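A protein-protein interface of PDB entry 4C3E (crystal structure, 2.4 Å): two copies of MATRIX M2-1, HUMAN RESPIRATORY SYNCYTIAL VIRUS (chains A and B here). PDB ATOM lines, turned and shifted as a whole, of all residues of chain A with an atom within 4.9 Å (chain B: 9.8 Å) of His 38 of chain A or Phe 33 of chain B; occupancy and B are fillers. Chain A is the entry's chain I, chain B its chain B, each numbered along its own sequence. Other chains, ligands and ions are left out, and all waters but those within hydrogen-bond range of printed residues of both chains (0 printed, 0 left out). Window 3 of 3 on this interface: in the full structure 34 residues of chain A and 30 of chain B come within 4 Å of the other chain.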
ATOM      1  N   LYS A  13       0.138 -16.614 -33.119  1.00  0.00           N
ATOM      2  CA  LYS A  13       1.208 -15.653 -32.815  1.00  0.00           C
ATOM      3  C   LYS A  13       0.738 -14.233 -32.924  1.00  0.00           C
ATOM      4  O   LYS A  13       1.208 -13.380 -32.176  1.00  0.00           O
ATOM      5  CB  LYS A  13       2.448 -15.914 -33.664  1.00  0.00           C
ATOM      6  CG  LYS A  13       3.167 -17.201 -33.203  1.00  0.00           C
ATOM      7  CD  LYS A  13       4.327 -17.716 -34.075  1.00  0.00           C
ATOM      8  CE  LYS A  13       5.636 -16.886 -33.999  1.00  0.00           C
ATOM      9  NZ  LYS A  13       5.871 -16.137 -32.715  1.00  0.00           N
ATOM     10  N   ILE A  16      -1.118 -13.844 -29.474  1.00  0.00           N
ATOM     11  CA  ILE A  16      -0.091 -13.698 -28.475  1.00  0.00           C
ATOM     12  C   ILE A  16       0.416 -12.265 -28.302  1.00  0.00           C
ATOM     13  O   ILE A  16       0.652 -11.857 -27.195  1.00  0.00           O
ATOM     14  CB  ILE A  16       1.092 -14.617 -28.693  1.00  0.00           C
ATOM     15  CG1 ILE A  16       0.654 -16.044 -28.541  1.00  0.00           C
ATOM     16  CG2 ILE A  16       2.122 -14.325 -27.613  1.00  0.00           C
ATOM     17  CD1 ILE A  16       1.730 -17.052 -28.830  1.00  0.00           C
ATOM     18  N   ARG A  17       0.434 -11.475 -29.352  1.00  0.00           N
ATOM     19  CA  ARG A  17       0.806 -10.076 -29.226  1.00  0.00           C
ATOM     20  C   ARG A  17      -0.292  -9.132 -29.100  1.00  0.00           C
ATOM     21  O   ARG A  17      -0.052  -7.919 -29.142  1.00  0.00           O
ATOM     22  CB  ARG A  17       1.532  -9.608 -30.494  1.00  0.00           C
ATOM     23  CG  ARG A  17       2.791 -10.384 -30.740  1.00  0.00           C
ATOM     24  CD  ARG A  17       3.392  -9.949 -32.064  1.00  0.00           C
ATOM     25  NE  ARG A  17       4.760 -10.359 -31.987  1.00  0.00           N
ATOM     26  CZ  ARG A  17       5.731  -9.585 -31.564  1.00  0.00           C
ATOM     27  NH1 ARG A  17       5.498  -8.296 -31.260  1.00  0.00           N
ATOM     28  NH2 ARG A  17       6.951 -10.115 -31.496  1.00  0.00           N
ATOM     29  N   PRO A  36      -0.831 -23.277 -23.963  1.00  0.00           N
ATOM     30  CA  PRO A  36       0.095 -23.533 -22.883  1.00  0.00           C
ATOM     31  C   PRO A  36       0.311 -22.252 -22.021  1.00  0.00           C
ATOM     32  O   PRO A  36       0.155 -21.126 -22.517  1.00  0.00           O
ATOM     33  CB  PRO A  36       1.402 -23.863 -23.608  1.00  0.00           C
ATOM     34  CG  PRO A  36       1.092 -23.843 -25.065  1.00  0.00           C
ATOM     35  CD  PRO A  36      -0.154 -23.049 -25.242  1.00  0.00           C
ATOM     36  N   PRO A  37       0.685 -22.445 -20.759  1.00  0.00           N
ATOM     37  CA  PRO A  37       0.889 -21.340 -19.837  1.00  0.00           C
ATOM     38  C   PRO A  37       1.904 -20.299 -20.319  1.00  0.00           C
ATOM     39  O   PRO A  37       1.642 -19.094 -20.237  1.00  0.00           O
ATOM     40  CB  PRO A  37       1.369 -22.001 -18.527  1.00  0.00           C
ATOM     41  CG  PRO A  37       1.466 -23.439 -18.776  1.00  0.00           C
ATOM     42  CD  PRO A  37       0.912 -23.765 -20.145  1.00  0.00           C
ATOM     43  N   HIS A  38       2.984 -20.737 -20.944  1.00  0.00           N
ATOM     44  CA  HIS A  38       3.964 -19.740 -21.401  1.00  0.00           C
ATOM     45  C   HIS A  38       3.348 -18.736 -22.367  1.00  0.00           C
ATOM     46  O   HIS A  38       3.595 -17.524 -22.288  1.00  0.00           O
ATOM     47  CB  HIS A  38       5.194 -20.403 -21.989  1.00  0.00           C
ATOM     48  CG  HIS A  38       6.364 -19.481 -22.063  1.00  0.00           C
ATOM     49  ND1 HIS A  38       6.647 -18.738 -23.187  1.00  0.00           N
ATOM     50  CD2 HIS A  38       7.279 -19.125 -21.134  1.00  0.00           C
ATOM     51  CE1 HIS A  38       7.713 -17.990 -22.957  1.00  0.00           C
ATOM     52  NE2 HIS A  38       8.123 -18.215 -21.723  1.00  0.00           N
ATOM     53  N   ALA A  39       2.488 -19.201 -23.257  1.00  0.00           N
ATOM     54  CA  ALA A  39       1.924 -18.267 -24.226  1.00  0.00           C
ATOM     55  C   ALA A  39       0.970 -17.306 -23.584  1.00  0.00           C
ATOM     56  O   ALA A  39       0.864 -16.155 -24.011  1.00  0.00           O
ATOM     57  CB  ALA A  39       1.221 -19.023 -25.362  1.00  0.00           C
ATOM     58  N   LEU A  40       0.221 -17.795 -22.582  1.00  0.00           N
ATOM     59  CA  LEU A  40      -0.666 -16.906 -21.840  1.00  0.00           C
ATOM     60  C   LEU A  40       0.153 -15.861 -21.025  1.00  0.00           C
ATOM     61  O   LEU A  40      -0.203 -14.683 -20.988  1.00  0.00           O
ATOM     62  CB  LEU A  40      -1.560 -17.715 -20.931  1.00  0.00           C
ATOM     63  CG  LEU A  40      -2.564 -18.663 -21.653  1.00  0.00           C
ATOM     64  CD1 LEU A  40      -3.086 -19.710 -20.710  1.00  0.00           C
ATOM     65  CD2 LEU A  40      -3.687 -17.866 -22.251  1.00  0.00           C
ATOM     66  N   LEU A  41       1.304 -16.266 -20.504  1.00  0.00           N
ATOM     67  CA  LEU A  41       2.212 -15.288 -19.829  1.00  0.00           C
ATOM     68  C   LEU A  41       2.754 -14.277 -20.792  1.00  0.00           C
ATOM     69  O   LEU A  41       2.817 -13.105 -20.480  1.00  0.00           O
ATOM     70  CB  LEU A  41       3.357 -16.036 -19.175  1.00  0.00           C
ATOM     71  CG  LEU A  41       2.948 -16.873 -17.951  1.00  0.00           C
ATOM     72  CD1 LEU A  41       4.033 -17.828 -17.551  1.00  0.00           C
ATOM     73  CD2 LEU A  41       2.624 -15.952 -16.803  1.00  0.00           C
ATOM     74  N   VAL A  42       3.171 -14.698 -22.004  1.00  0.00           N
ATOM     75  CA  VAL A  42       3.763 -13.747 -22.956  1.00  0.00           C
ATOM     76  C   VAL A  42       2.727 -12.768 -23.401  1.00  0.00           C
ATOM     77  O   VAL A  42       2.964 -11.547 -23.475  1.00  0.00           O
ATOM     78  CB  VAL A  42       4.320 -14.471 -24.172  1.00  0.00           C
ATOM     79  CG1 VAL A  42       4.722 -13.480 -25.249  1.00  0.00           C
ATOM     80  CG2 VAL A  42       5.521 -15.313 -23.805  1.00  0.00           C
ATOM     81  N   PHE A  46       2.604  -8.470 -23.457  1.00  0.00           N
ATOM     82  CA  PHE A  46       2.348  -7.570 -24.575  1.00  0.00           C
ATOM     83  C   PHE A  46       1.123  -6.740 -24.326  1.00  0.00           C
ATOM     84  O   PHE A  46       1.087  -5.533 -24.651  1.00  0.00           O
ATOM     85  CB  PHE A  46       2.176  -8.374 -25.906  1.00  0.00           C
ATOM     86  CG  PHE A  46       3.468  -8.871 -26.486  1.00  0.00           C
ATOM     87  CD1 PHE A  46       4.442  -7.971 -26.950  1.00  0.00           C
ATOM     88  CD2 PHE A  46       3.743 -10.219 -26.525  1.00  0.00           C
ATOM     89  CE1 PHE A  46       5.662  -8.428 -27.479  1.00  0.00           C
ATOM     90  CE2 PHE A  46       4.976 -10.693 -27.009  1.00  0.00           C
ATOM     91  CZ  PHE A  46       5.939  -9.803 -27.500  1.00  0.00           C
ATOM     92  N   ARG B   8      21.892 -19.118 -23.581  1.00  0.00           N
ATOM     93  CA  ARG B   8      20.970 -17.988 -23.769  1.00  0.00           C
ATOM     94  C   ARG B   8      20.894 -16.955 -22.649  1.00  0.00           C
ATOM     95  O   ARG B   8      21.338 -17.087 -21.482  1.00  0.00           O
ATOM     96  CB  ARG B   8      19.557 -18.555 -23.890  1.00  0.00           C
ATOM     97  CG  ARG B   8      18.205 -18.036 -24.463  1.00  0.00           C
ATOM     98  CD  ARG B   8      17.062 -18.665 -23.624  1.00  0.00           C
ATOM     99  NE  ARG B   8      16.823 -20.058 -23.926  1.00  0.00           N
ATOM    100  CZ  ARG B   8      15.836 -20.765 -23.394  1.00  0.00           C
ATOM    101  NH1 ARG B   8      14.975 -20.179 -22.580  1.00  0.00           N
ATOM    102  NH2 ARG B   8      15.696 -22.049 -23.699  1.00  0.00           N
ATOM    103  N   ARG B   9      20.256 -15.890 -23.062  1.00  0.00           N
ATOM    104  CA  ARG B   9      20.314 -14.670 -22.307  1.00  0.00           C
ATOM    105  C   ARG B   9      19.305 -14.632 -21.149  1.00  0.00           C
ATOM    106  O   ARG B   9      18.135 -14.982 -21.322  1.00  0.00           O
ATOM    107  CB  ARG B   9      20.069 -13.480 -23.221  1.00  0.00           C
ATOM    108  CG  ARG B   9      21.194 -13.118 -24.158  1.00  0.00           C
ATOM    109  CD  ARG B   9      20.812 -11.951 -25.057  1.00  0.00           C
ATOM    110  NE  ARG B   9      21.664 -11.950 -26.241  1.00  0.00           N
ATOM    111  CZ  ARG B   9      22.941 -11.557 -26.260  1.00  0.00           C
ATOM    112  NH1 ARG B   9      23.542 -11.106 -25.159  1.00  0.00           N
ATOM    113  NH2 ARG B   9      23.625 -11.605 -27.400  1.00  0.00           N
ATOM    114  N   PRO B  11      16.889 -12.689 -18.483  1.00  0.00           N
ATOM    115  CA  PRO B  11      16.019 -11.576 -18.687  1.00  0.00           C
ATOM    116  C   PRO B  11      16.605 -10.312 -18.096  1.00  0.00           C
ATOM    117  O   PRO B  11      17.176 -10.334 -17.028  1.00  0.00           O
ATOM    118  CB  PRO B  11      14.741 -11.974 -17.956  1.00  0.00           C
ATOM    119  CG  PRO B  11      15.057 -13.199 -17.187  1.00  0.00           C
ATOM    120  CD  PRO B  11      16.251 -13.809 -17.801  1.00  0.00           C
ATOM    121  N   GLU B  15      13.677  -4.655 -17.389  1.00  0.00           N
ATOM    122  CA  GLU B  15      12.516  -4.888 -18.240  1.00  0.00           C
ATOM    123  C   GLU B  15      11.528  -5.601 -17.331  1.00  0.00           C
ATOM    124  O   GLU B  15      10.362  -5.309 -17.349  1.00  0.00           O
ATOM    125  CB  GLU B  15      12.887  -5.763 -19.447  1.00  0.00           C
ATOM    126  CG  GLU B  15      11.782  -6.035 -20.478  1.00  0.00           C
ATOM    127  CD  GLU B  15      11.373  -4.836 -21.236  1.00  0.00           C
ATOM    128  OE1 GLU B  15      12.137  -3.864 -21.270  1.00  0.00           O
ATOM    129  OE2 GLU B  15      10.244  -4.831 -21.812  1.00  0.00           O
ATOM    130  N   SER B  29      18.129 -10.154 -22.083  1.00  0.00           N
ATOM    131  CA  SER B  29      16.993 -10.407 -22.961  1.00  0.00           C
ATOM    132  C   SER B  29      15.837  -9.505 -22.707  1.00  0.00           C
ATOM    133  O   SER B  29      15.399  -9.399 -21.587  1.00  0.00           O
ATOM    134  CB  SER B  29      16.473 -11.834 -22.833  1.00  0.00           C
ATOM    135  OG  SER B  29      15.269 -11.927 -23.615  1.00  0.00           O
ATOM    136  N   HIS B  30      15.305  -8.928 -23.766  1.00  0.00           N
ATOM    137  CA  HIS B  30      14.119  -8.160 -23.747  1.00  0.00           C
ATOM    138  C   HIS B  30      13.034  -8.892 -24.513  1.00  0.00           C
ATOM    139  O   HIS B  30      12.030  -8.300 -24.915  1.00  0.00           O
ATOM    140  CB  HIS B  30      14.374  -6.778 -24.341  1.00  0.00           C
ATOM    141  CG  HIS B  30      15.494  -6.063 -23.653  1.00  0.00           C
ATOM    142  ND1 HIS B  30      16.812  -6.251 -24.006  1.00  0.00           N
ATOM    143  CD2 HIS B  30      15.509  -5.259 -22.568  1.00  0.00           C
ATOM    144  CE1 HIS B  30      17.581  -5.546 -23.211  1.00  0.00           C
ATOM    145  NE2 HIS B  30      16.813  -4.917 -22.341  1.00  0.00           N
ATOM    146  N   ASN B  31      13.249 -10.165 -24.748  1.00  0.00           N
ATOM    147  CA  ASN B  31      12.357 -10.916 -25.616  1.00  0.00           C
ATOM    148  C   ASN B  31      11.513 -11.894 -24.783  1.00  0.00           C
ATOM    149  O   ASN B  31      12.012 -12.939 -24.344  1.00  0.00           O
ATOM    150  CB  ASN B  31      13.176 -11.696 -26.625  1.00  0.00           C
ATOM    151  CG  ASN B  31      12.322 -12.655 -27.452  1.00  0.00           C
ATOM    152  OD1 ASN B  31      11.126 -12.459 -27.618  1.00  0.00           O
ATOM    153  ND2 ASN B  31      12.957 -13.647 -28.017  1.00  0.00           N
ATOM    154  N   TYR B  32      10.259 -11.540 -24.546  1.00  0.00           N
ATOM    155  CA  TYR B  32       9.416 -12.316 -23.615  1.00  0.00           C
ATOM    156  C   TYR B  32       9.309 -13.812 -23.979  1.00  0.00           C
ATOM    157  O   TYR B  32       9.195 -14.644 -23.086  1.00  0.00           O
ATOM    158  CB  TYR B  32       8.050 -11.715 -23.508  1.00  0.00           C
ATOM    159  CG  TYR B  32       8.042 -10.227 -23.235  1.00  0.00           C
ATOM    160  CD1 TYR B  32       8.920  -9.633 -22.302  1.00  0.00           C
ATOM    161  CD2 TYR B  32       7.176  -9.436 -23.835  1.00  0.00           C
ATOM    162  CE1 TYR B  32       8.929  -8.245 -22.096  1.00  0.00           C
ATOM    163  CE2 TYR B  32       7.146  -8.048 -23.588  1.00  0.00           C
ATOM    164  CZ  TYR B  32       8.060  -7.473 -22.717  1.00  0.00           C
ATOM    165  OH  TYR B  32       7.989  -6.127 -22.485  1.00  0.00           O
ATOM    166  N   PHE B  33       9.426 -14.138 -25.266  1.00  0.00           N
ATOM    167  CA  PHE B  33       9.348 -15.536 -25.721  1.00  0.00           C
ATOM    168  C   PHE B  33      10.437 -16.374 -25.155  1.00  0.00           C
ATOM    169  O   PHE B  33      10.319 -17.547 -25.125  1.00  0.00           O
ATOM    170  CB  PHE B  33       9.382 -15.652 -27.269  1.00  0.00           C
ATOM    171  CG  PHE B  33       8.166 -15.067 -27.932  1.00  0.00           C
ATOM    172  CD1 PHE B  33       7.030 -15.834 -28.117  1.00  0.00           C
ATOM    173  CD2 PHE B  33       8.152 -13.778 -28.391  1.00  0.00           C
ATOM    174  CE1 PHE B  33       5.917 -15.292 -28.704  1.00  0.00           C
ATOM    175  CE2 PHE B  33       7.012 -13.214 -28.979  1.00  0.00           C
ATOM    176  CZ  PHE B  33       5.903 -13.967 -29.127  1.00  0.00           C
ATOM    177  N   GLU B  34      11.538 -15.800 -24.748  1.00  0.00           N
ATOM    178  CA  GLU B  34      12.588 -16.638 -24.198  1.00  0.00           C
ATOM    179  C   GLU B  34      12.706 -16.545 -22.668  1.00  0.00           C
ATOM    180  O   GLU B  34      13.571 -17.161 -22.072  1.00  0.00           O
ATOM    181  CB  GLU B  34      13.930 -16.367 -24.898  1.00  0.00           C
ATOM    182  CG  GLU B  34      14.529 -14.965 -24.741  1.00  0.00           C
ATOM    183  CD  GLU B  34      15.737 -14.682 -25.665  1.00  0.00           C
ATOM    184  OE1 GLU B  34      15.936 -15.413 -26.668  1.00  0.00           O
ATOM    185  OE2 GLU B  34      16.478 -13.692 -25.400  1.00  0.00           O
ATOM    186  N   TRP B  35      11.858 -15.761 -22.022  1.00  0.00           N
ATOM    187  CA  TRP B  35      11.948 -15.598 -20.559  1.00  0.00           C
ATOM    188  C   TRP B  35      11.442 -16.815 -19.846  1.00  0.00           C
ATOM    189  O   TRP B  35      10.440 -17.429 -20.277  1.00  0.00           O
ATOM    190  CB  TRP B  35      11.142 -14.403 -20.149  1.00  0.00           C
ATOM    191  CG  TRP B  35      11.779 -13.133 -20.407  1.00  0.00           C
ATOM    192  CD1 TRP B  35      12.813 -12.891 -21.257  1.00  0.00           C
ATOM    193  CD2 TRP B  35      11.488 -11.890 -19.761  1.00  0.00           C
ATOM    194  NE1 TRP B  35      13.139 -11.572 -21.225  1.00  0.00           N
ATOM    195  CE2 TRP B  35      12.364 -10.936 -20.297  1.00  0.00           C
ATOM    196  CE3 TRP B  35      10.569 -11.486 -18.800  1.00  0.00           C
ATOM    197  CZ2 TRP B  35      12.358  -9.601 -19.885  1.00  0.00           C
ATOM    198  CZ3 TRP B  35      10.551 -10.157 -18.399  1.00  0.00           C
ATOM    199  CH2 TRP B  35      11.426  -9.231 -18.946  1.00  0.00           C
ATOM    200  N   PRO B  36      12.072 -17.173 -18.744  1.00  0.00           N
ATOM    201  CA  PRO B  36      11.336 -18.106 -17.850  1.00  0.00           C
ATOM    202  C   PRO B  36      10.004 -17.536 -17.292  1.00  0.00           C
ATOM    203  O   PRO B  36       9.819 -16.327 -17.185  1.00  0.00           O
ATOM    204  CB  PRO B  36      12.292 -18.317 -16.679  1.00  0.00           C
ATOM    205  CG  PRO B  36      13.520 -17.485 -16.968  1.00  0.00           C
ATOM    206  CD  PRO B  36      13.114 -16.462 -17.985  1.00  0.00           C
ATOM    207  N   PRO B  37       9.041 -18.417 -16.988  1.00  0.00           N
ATOM    208  CA  PRO B  37       7.754 -17.978 -16.549  1.00  0.00           C
ATOM    209  C   PRO B  37       7.829 -17.079 -15.324  1.00  0.00           C
ATOM    210  O   PRO B  37       7.069 -16.128 -15.203  1.00  0.00           O
ATOM    211  CB  PRO B  37       6.995 -19.287 -16.236  1.00  0.00           C
ATOM    212  CG  PRO B  37       7.915 -20.406 -16.513  1.00  0.00           C
ATOM    213  CD  PRO B  37       9.172 -19.873 -17.127  1.00  0.00           C
ATOM    214  N   HIS B  38       8.706 -17.376 -14.381  1.00  0.00           N
ATOM    215  CA  HIS B  38       8.718 -16.581 -13.150  1.00  0.00           C
ATOM    216  C   HIS B  38       8.984 -15.123 -13.460  1.00  0.00           C
ATOM    217  O   HIS B  38       8.324 -14.227 -12.902  1.00  0.00           O
ATOM    218  CB  HIS B  38       9.712 -17.115 -12.142  1.00  0.00           C
ATOM    219  CG  HIS B  38       9.476 -16.575 -10.782  1.00  0.00           C
ATOM    220  ND1 HIS B  38      10.199 -15.519 -10.268  1.00  0.00           N
ATOM    221  CD2 HIS B  38       8.583 -16.938  -9.829  1.00  0.00           C
ATOM    222  CE1 HIS B  38       9.752 -15.240  -9.067  1.00  0.00           C
ATOM    223  NE2 HIS B  38       8.798 -16.112  -8.761  1.00  0.00           N
ATOM    224  N   ALA B  39       9.863 -14.859 -14.426  1.00  0.00           N
ATOM    225  CA  ALA B  39      10.153 -13.482 -14.731  1.00  0.00           C
ATOM    226  C   ALA B  39       9.009 -12.791 -15.408  1.00  0.00           C
ATOM    227  O   ALA B  39       8.749 -11.602 -15.174  1.00  0.00           O
ATOM    228  CB  ALA B  39      11.388 -13.386 -15.607  1.00  0.00           C
ATOM    229  N   LEU B  40       8.273 -13.530 -16.232  1.00  0.00           N
ATOM    230  CA  LEU B  40       7.062 -12.963 -16.830  1.00  0.00           C
ATOM    231  C   LEU B  40       5.989 -12.691 -15.750  1.00  0.00           C
ATOM    232  O   LEU B  40       5.282 -11.678 -15.806  1.00  0.00           O
ATOM    233  CB  LEU B  40       6.522 -13.903 -17.942  1.00  0.00           C
ATOM    234  CG  LEU B  40       7.489 -14.080 -19.138  1.00  0.00           C
ATOM    235  CD1 LEU B  40       7.100 -15.295 -19.961  1.00  0.00           C
ATOM    236  CD2 LEU B  40       7.483 -12.859 -20.022  1.00  0.00           C
ATOM    237  N   LEU B  41       5.864 -13.583 -14.778  1.00  0.00           N
ATOM    238  CA  LEU B  41       4.957 -13.331 -13.637  1.00  0.00           C
ATOM    239  C   LEU B  41       5.320 -12.130 -12.815  1.00  0.00           C
ATOM    240  O   LEU B  41       4.456 -11.307 -12.472  1.00  0.00           O
ATOM    241  CB  LEU B  41       4.915 -14.531 -12.737  1.00  0.00           C
ATOM    242  CG  LEU B  41       4.211 -15.733 -13.351  1.00  0.00           C
ATOM    243  CD1 LEU B  41       4.491 -17.000 -12.570  1.00  0.00           C
ATOM    244  CD2 LEU B  41       2.713 -15.501 -13.377  1.00  0.00           C
ATOM    245  N   GLN B  44       4.568  -8.813 -14.760  1.00  0.00           N
ATOM    246  CA  GLN B  44       3.128  -8.469 -14.813  1.00  0.00           C
ATOM    247  C   GLN B  44       2.716  -7.730 -13.565  1.00  0.00           C
ATOM    248  O   GLN B  44       1.983  -6.745 -13.616  1.00  0.00           O
ATOM    249  CB  GLN B  44       2.290  -9.699 -14.883  1.00  0.00           C
ATOM    250  CG  GLN B  44       2.327 -10.295 -16.250  1.00  0.00           C
ATOM    251  CD  GLN B  44       1.818 -11.724 -16.210  1.00  0.00           C
ATOM    252  OE1 GLN B  44       0.834 -11.982 -15.558  1.00  0.00           O
ATOM    253  NE2 GLN B  44       2.485 -12.641 -16.906  1.00  0.00           N
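His 38 of chain A touches Leu 40 of chain B, but with the chains exchanged Leu 40 of chain A does not touch His 38 of chain B (10.9 Å). Leu 41 of chain A touches Pro 37 of chain B, but with the chains exchanged Pro 37 of chain A does not touch Leu 41 of chain B (7.8 Å). Leu 41 of chain A touches Leu 40 of chain B, but with the chains exchanged Leu 40 of chain A does not touch Leu 41 of chain B (8.1 Å). Leu 41 of chain A touches its own counterpart, Leu 41 of chain B.
Among the printed residues, 12 pairs touch across the chains. Among the printed residues, no Asp or Glu carboxylate lies within 4 Å of a Lys or Arg side-chain nitrogen of the other chain.
O of Trp 35 of chain B sits at hydrogen-bond distance from NE2 of His 38 of chain A (2.8 Å).
His 38 of chain A touches just these residues of chain B: Tyr 32 (3.7 Å), Phe 33 (3.4 Å), Trp 35 (2.8 Å) and Leu 40 (3.6 Å). Of the printed residues of chain A, Phe 33 of chain B touches Arg 17 (3.99 Å), His 38 (3.4 Å) and Phe 46 (3.8 Å). No residue of chain B comes within 4 Å of Pro 37 of chain A. No residue of chain B comes within 4 Å of Ala 39 of chain A. Of the printed residues of chain B, Arg 17 of chain A touches Phe 33. Printed residues of chain A within 4 Å of Trp 35 of chain B: His 38. Printed residues of chain B within 4 Å of Phe 46 of chain A: Tyr 32 and Phe 33. Of the printed residues of chain B, Leu 41 of chain A touches Pro 37 (3.6 Å), Leu 40 (3.9 Å), Leu 41 (3.5 Å) and Gln 44 (3.3 Å). Of the printed residues of chain A, Tyr 32 of chain B touches His 38 (3.7 Å), Val 42 (3.8 Å) and Phe 46 (3.9 Å). Leu 40 of chain A touches none of the printed residues of chain B. The nearest residue of chain B that does not touch His 38 of chain A is Pro 37 of chain B (4.5 Å).
Among the printed residues, pairs that only touch across the chains: Leu 41 of chain A with Gln 44 of chain B (3.3 Å), His 38 of chain A with Phe 33 of chain B (3.4 Å), Leu 41 of chain A with Leu 41 of chain B (3.5 Å), Leu 41 of chain A with Pro 37 of chain B (3.6 Å), His 38 of chain A with Leu 40 of chain B (3.6 Å), His 38 of chain A with Tyr 32 of chain B (3.7 Å), Phe 46 of chain A with Phe 33 of chain B (3.8 Å), Val 42 of chain A with Tyr 32 of chain B (3.8 Å), Phe 46 of chain A with Tyr 32 of chain B (3.9 Å), Leu 41 of chain A with Leu 40 of chain B (3.9 Å) and Arg 17 of chain A with Phe 33 of chain B (3.99 Å).
The side-chain amide oxygen (OD1) of Asn 31 of chain B lies close to the backbone NH (N) of Phe 33 of chain B, 3.4 Å away. The side-chain amide nitrogen (NE2) of Gln 44 of chain B is in hydrogen-bond range of the backbone carbonyl oxygen (O) of Leu 40 of chain B. The side-chain carboxylate of Glu 15 of chain B sits at hydrogen-bond distance from the side-chain hydroxyl of Tyr 32 of chain B, 2.7 Å away. The backbone carbonyl oxygen of Ser 29 of chain B sits at hydrogen-bond distance from the indole nitrogen of Trp 35 of chain B (3.2 Å).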
